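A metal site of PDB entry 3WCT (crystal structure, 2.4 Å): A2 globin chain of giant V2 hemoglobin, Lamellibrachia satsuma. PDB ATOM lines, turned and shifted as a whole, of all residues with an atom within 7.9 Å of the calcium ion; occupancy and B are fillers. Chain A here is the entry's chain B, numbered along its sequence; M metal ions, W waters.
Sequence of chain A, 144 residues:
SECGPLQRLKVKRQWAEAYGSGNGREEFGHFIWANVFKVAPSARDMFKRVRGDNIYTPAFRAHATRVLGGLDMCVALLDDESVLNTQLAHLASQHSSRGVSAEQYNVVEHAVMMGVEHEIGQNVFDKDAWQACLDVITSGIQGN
The calcium ion is bound by the side-chain carboxylate (OD1) of Asp 135, water W1, water W2, the side-chain carboxylate (OE2) of Glu 109, the side-chain amide oxygen (OD1) of Asn 106 and the side-chain carboxylate (OE1) of Glu 109.
Of the 16 residues printed, 3 come within 4 Å of the calcium ion.
Along chain A the residues within 4 Å of the calcium ion span positions 106 to 135.
OD1 of Asp 135 sits close to OE1 of Gln 131 (3.5 Å).
The side-chain hydroxyl of Thr 138 sits at hydrogen-bond distance from the backbone carbonyl oxygen of Asp 135.
OG1 of Thr 138 lies close to OE2 of Glu 109.
The side-chain carboxylate (OE1) of Glu 109 lies close to the side-chain amide oxygen (OE1) of Gln 131 (2.6 Å).
The backbone carbonyl oxygen of Ala 102 is in hydrogen-bond range of the side-chain amide nitrogen of Asn 106, 2.9 Å away.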
ATOM      1  N   ALA A 102       7.913 -10.207   2.425  1.00  0.00           N
ATOM      2  CA  ALA A 102       6.521 -10.426   2.797  1.00  0.00           C
ATOM      3  C   ALA A 102       6.064 -11.803   2.338  1.00  0.00           C
ATOM      4  O   ALA A 102       5.064 -12.328   2.834  1.00  0.00           O
ATOM      5  CB  ALA A 102       5.635  -9.359   2.164  1.00  0.00           C
ATOM      6  N   GLU A 103       6.793 -12.398   1.398  1.00  0.00           N
ATOM      7  CA  GLU A 103       6.454 -13.722   0.892  1.00  0.00           C
ATOM      8  C   GLU A 103       6.842 -14.775   1.918  1.00  0.00           C
ATOM      9  O   GLU A 103       6.093 -15.713   2.177  1.00  0.00           O
ATOM     10  CB  GLU A 103       7.194 -13.990  -0.419  1.00  0.00           C
ATOM     11  CG  GLU A 103       6.531 -15.035  -1.313  1.00  0.00           C
ATOM     12  CD  GLU A 103       5.605 -14.420  -2.348  1.00  0.00           C
ATOM     13  OE1 GLU A 103       6.114 -13.715  -3.254  1.00  0.00           O
ATOM     14  OE2 GLU A 103       4.371 -14.623  -2.265  1.00  0.00           O
ATOM     15  N   TYR A 105       7.155 -14.249   5.056  1.00  0.00           N
ATOM     16  CA  TYR A 105       6.327 -14.064   6.235  1.00  0.00           C
ATOM     17  C   TYR A 105       5.059 -14.881   6.050  1.00  0.00           C
ATOM     18  O   TYR A 105       4.650 -15.608   6.954  1.00  0.00           O
ATOM     19  CB  TYR A 105       5.981 -12.582   6.433  1.00  0.00           C
ATOM     20  CG  TYR A 105       7.021 -11.864   7.248  1.00  0.00           C
ATOM     21  CD1 TYR A 105       7.256 -12.228   8.570  1.00  0.00           C
ATOM     22  CD2 TYR A 105       7.815 -10.865   6.687  1.00  0.00           C
ATOM     23  CE1 TYR A 105       8.253 -11.609   9.321  1.00  0.00           C
ATOM     24  CE2 TYR A 105       8.825 -10.242   7.433  1.00  0.00           C
ATOM     25  CZ  TYR A 105       9.036 -10.624   8.748  1.00  0.00           C
ATOM     26  OH  TYR A 105      10.055 -10.050   9.491  1.00  0.00           O
ATOM     27  N   ASN A 106       4.469 -14.777   4.858  1.00  0.00           N
ATOM     28  CA  ASN A 106       3.272 -15.535   4.552  1.00  0.00           C
ATOM     29  C   ASN A 106       3.545 -17.037   4.634  1.00  0.00           C
ATOM     30  O   ASN A 106       2.680 -17.795   5.060  1.00  0.00           O
ATOM     31  CB  ASN A 106       2.741 -15.196   3.157  1.00  0.00           C
ATOM     32  CG  ASN A 106       2.284 -13.754   3.033  1.00  0.00           C
ATOM     33  OD1 ASN A 106       1.768 -13.172   3.991  1.00  0.00           O
ATOM     34  ND2 ASN A 106       2.443 -13.179   1.835  1.00  0.00           N
ATOM     35  N   VAL A 107       4.740 -17.463   4.236  1.00  0.00           N
ATOM     36  CA  VAL A 107       5.080 -18.876   4.300  1.00  0.00           C
ATOM     37  C   VAL A 107       4.947 -19.367   5.730  1.00  0.00           C
ATOM     38  O   VAL A 107       4.202 -20.309   6.013  1.00  0.00           O
ATOM     39  CB  VAL A 107       6.515 -19.153   3.834  1.00  0.00           C
ATOM     40  CG1 VAL A 107       6.906 -20.591   4.183  1.00  0.00           C
ATOM     41  CG2 VAL A 107       6.644 -18.907   2.338  1.00  0.00           C
ATOM     42  N   GLU A 109       3.405 -18.137   8.057  1.00  0.00           N
ATOM     43  CA  GLU A 109       2.007 -18.034   8.490  1.00  0.00           C
ATOM     44  C   GLU A 109       1.305 -19.357   8.210  1.00  0.00           C
ATOM     45  O   GLU A 109       0.692 -19.944   9.101  1.00  0.00           O
ATOM     46  CB  GLU A 109       1.266 -16.917   7.720  1.00  0.00           C
ATOM     47  CG  GLU A 109       1.532 -15.499   8.185  1.00  0.00           C
ATOM     48  CD  GLU A 109       0.807 -14.480   7.323  1.00  0.00           C
ATOM     49  OE1 GLU A 109      -0.342 -14.754   6.914  1.00  0.00           O
ATOM     50  OE2 GLU A 109       1.374 -13.394   7.053  1.00  0.00           O
ATOM     51  N   HIS A 110       1.386 -19.819   6.959  1.00  0.00           N
ATOM     52  CA  HIS A 110       0.768 -21.080   6.552  1.00  0.00           C
ATOM     53  C   HIS A 110       1.355 -22.205   7.396  1.00  0.00           C
ATOM     54  O   HIS A 110       0.618 -23.049   7.914  1.00  0.00           O
ATOM     55  CB  HIS A 110       0.991 -21.314   5.039  1.00  0.00           C
ATOM     56  CG  HIS A 110       0.288 -22.524   4.496  1.00  0.00           C
ATOM     57  ND1 HIS A 110       0.916 -23.740   4.318  1.00  0.00           N
ATOM     58  CD2 HIS A 110      -0.995 -22.700   4.086  1.00  0.00           C
ATOM     59  CE1 HIS A 110       0.054 -24.616   3.825  1.00  0.00           C
ATOM     60  NE2 HIS A 110      -1.111 -24.016   3.677  1.00  0.00           N
ATOM     61  N   MET A 113      -0.220 -22.160  10.750  1.00  0.00           N
ATOM     62  CA  MET A 113      -1.593 -22.603  10.709  1.00  0.00           C
ATOM     63  C   MET A 113      -1.688 -24.125  10.610  1.00  0.00           C
ATOM     64  O   MET A 113      -2.421 -24.748  11.375  1.00  0.00           O
ATOM     65  CB  MET A 113      -2.348 -21.950   9.550  1.00  0.00           C
ATOM     66  CG  MET A 113      -2.433 -20.426   9.659  1.00  0.00           C
ATOM     67  SD  MET A 113      -3.705 -19.666   8.589  1.00  0.00           S
ATOM     68  CE  MET A 113      -2.746 -19.154   7.260  1.00  0.00           C
ATOM     69  N   GLN A 131      -5.771 -16.552  10.021  1.00  0.00           N
ATOM     70  CA  GLN A 131      -5.163 -15.825   8.918  1.00  0.00           C
ATOM     71  C   GLN A 131      -5.248 -14.328   9.195  1.00  0.00           C
ATOM     72  O   GLN A 131      -4.264 -13.614   9.055  1.00  0.00           O
ATOM     73  CB  GLN A 131      -5.879 -16.159   7.608  1.00  0.00           C
ATOM     74  CG  GLN A 131      -5.232 -15.581   6.342  1.00  0.00           C
ATOM     75  CD  GLN A 131      -3.816 -16.074   6.118  1.00  0.00           C
ATOM     76  OE1 GLN A 131      -2.850 -15.572   6.725  1.00  0.00           O
ATOM     77  NE2 GLN A 131      -3.672 -17.074   5.236  1.00  0.00           N
ATOM     78  N   ALA A 132      -6.426 -13.857   9.614  1.00  0.00           N
ATOM     79  CA  ALA A 132      -6.606 -12.433   9.910  1.00  0.00           C
ATOM     80  C   ALA A 132      -5.625 -11.981  10.994  1.00  0.00           C
ATOM     81  O   ALA A 132      -4.885 -11.010  10.814  1.00  0.00           O
ATOM     82  CB  ALA A 132      -8.042 -12.176  10.350  1.00  0.00           C
ATOM     83  N   LEU A 134      -2.921 -13.434  12.030  1.00  0.00           N
ATOM     84  CA  LEU A 134      -1.508 -13.675  11.714  1.00  0.00           C
ATOM     85  C   LEU A 134      -1.084 -12.540  10.772  1.00  0.00           C
ATOM     86  O   LEU A 134       0.060 -12.092  10.808  1.00  0.00           O
ATOM     87  CB  LEU A 134      -1.289 -15.041  11.050  1.00  0.00           C
ATOM     88  CG  LEU A 134      -1.216 -16.293  11.939  1.00  0.00           C
ATOM     89  CD1 LEU A 134      -0.901 -17.518  11.078  1.00  0.00           C
ATOM     90  CD2 LEU A 134      -0.119 -16.114  12.997  1.00  0.00           C
ATOM     91  N   ASP A 135      -2.013 -12.074   9.927  1.00  0.00           N
ATOM     92  CA  ASP A 135      -1.708 -10.964   9.025  1.00  0.00           C
ATOM     93  C   ASP A 135      -1.365  -9.765   9.922  1.00  0.00           C
ATOM     94  O   ASP A 135      -0.341  -9.104   9.727  1.00  0.00           O
ATOM     95  CB  ASP A 135      -2.920 -10.610   8.144  1.00  0.00           C
ATOM     96  CG  ASP A 135      -3.136 -11.588   6.998  1.00  0.00           C
ATOM     97  OD1 ASP A 135      -2.150 -12.176   6.499  1.00  0.00           O
ATOM     98  OD2 ASP A 135      -4.302 -11.761   6.583  1.00  0.00           O
ATOM     99  N   VAL A 136      -2.222  -9.521  10.906  1.00  0.00           N
ATOM    100  CA  VAL A 136      -2.012  -8.430  11.862  1.00  0.00           C
ATOM    101  C   VAL A 136      -0.653  -8.539  12.528  1.00  0.00           C
ATOM    102  O   VAL A 136       0.032  -7.538  12.752  1.00  0.00           O
ATOM    103  CB  VAL A 136      -3.115  -8.434  12.974  1.00  0.00           C
ATOM    104  CG1 VAL A 136      -2.700  -7.559  14.152  1.00  0.00           C
ATOM    105  CG2 VAL A 136      -4.438  -7.933  12.401  1.00  0.00           C
ATOM    106  N   THR A 138       2.336 -10.403  11.486  1.00  0.00           N
ATOM    107  CA  THR A 138       3.479 -10.269  10.591  1.00  0.00           C
ATOM    108  C   THR A 138       3.529  -8.866   9.999  1.00  0.00           C
ATOM    109  O   THR A 138       4.591  -8.246   9.878  1.00  0.00           O
ATOM    110  CB  THR A 138       3.416 -11.271   9.437  1.00  0.00           C
ATOM    111  OG1 THR A 138       2.237 -11.023   8.675  1.00  0.00           O
ATOM    112  CG2 THR A 138       3.374 -12.688   9.974  1.00  0.00           C
ATOM    113  N   SER A 139       2.355  -8.371   9.612  1.00  0.00           N
ATOM    114  CA  SER A 139       2.204  -7.030   9.057  1.00  0.00           C
ATOM    115  C   SER A 139       2.889  -6.036   9.988  1.00  0.00           C
ATOM    116  O   SER A 139       3.514  -5.078   9.537  1.00  0.00           O
ATOM    117  CB  SER A 139       0.719  -6.696   8.913  1.00  0.00           C
ATOM    118  OG  SER A 139       0.524  -5.329   8.603  1.00  0.00           O
ATOM    119  N   GLN A 142       6.763  -6.353  10.080  1.00  0.00           N
ATOM    120  CA  GLN A 142       7.357  -5.771   8.871  1.00  0.00           C
ATOM    121  C   GLN A 142       7.138  -4.262   8.897  1.00  0.00           C
ATOM    122  O   GLN A 142       7.050  -3.632   7.842  1.00  0.00           O
ATOM    123  CB  GLN A 142       6.687  -6.313   7.597  1.00  0.00           C
ATOM    124  CG  GLN A 142       6.657  -7.800   7.432  1.00  0.00           C
ATOM    125  CD  GLN A 142       6.051  -8.215   6.100  1.00  0.00           C
ATOM    126  OE1 GLN A 142       6.687  -8.093   5.053  1.00  0.00           O
ATOM    127  NE2 GLN A 142       4.822  -8.691   6.139  1.00  0.00           N
HETATM  128 CA    CA M   1      -0.117 -12.597   5.362  1.00  0.00          CA
HETATM  129  O   HOH W   1      -1.275 -14.070   3.905  1.00  0.00           O
HETATM  130  O   HOH W   2       1.173 -10.959   6.526  1.00  0.00           O
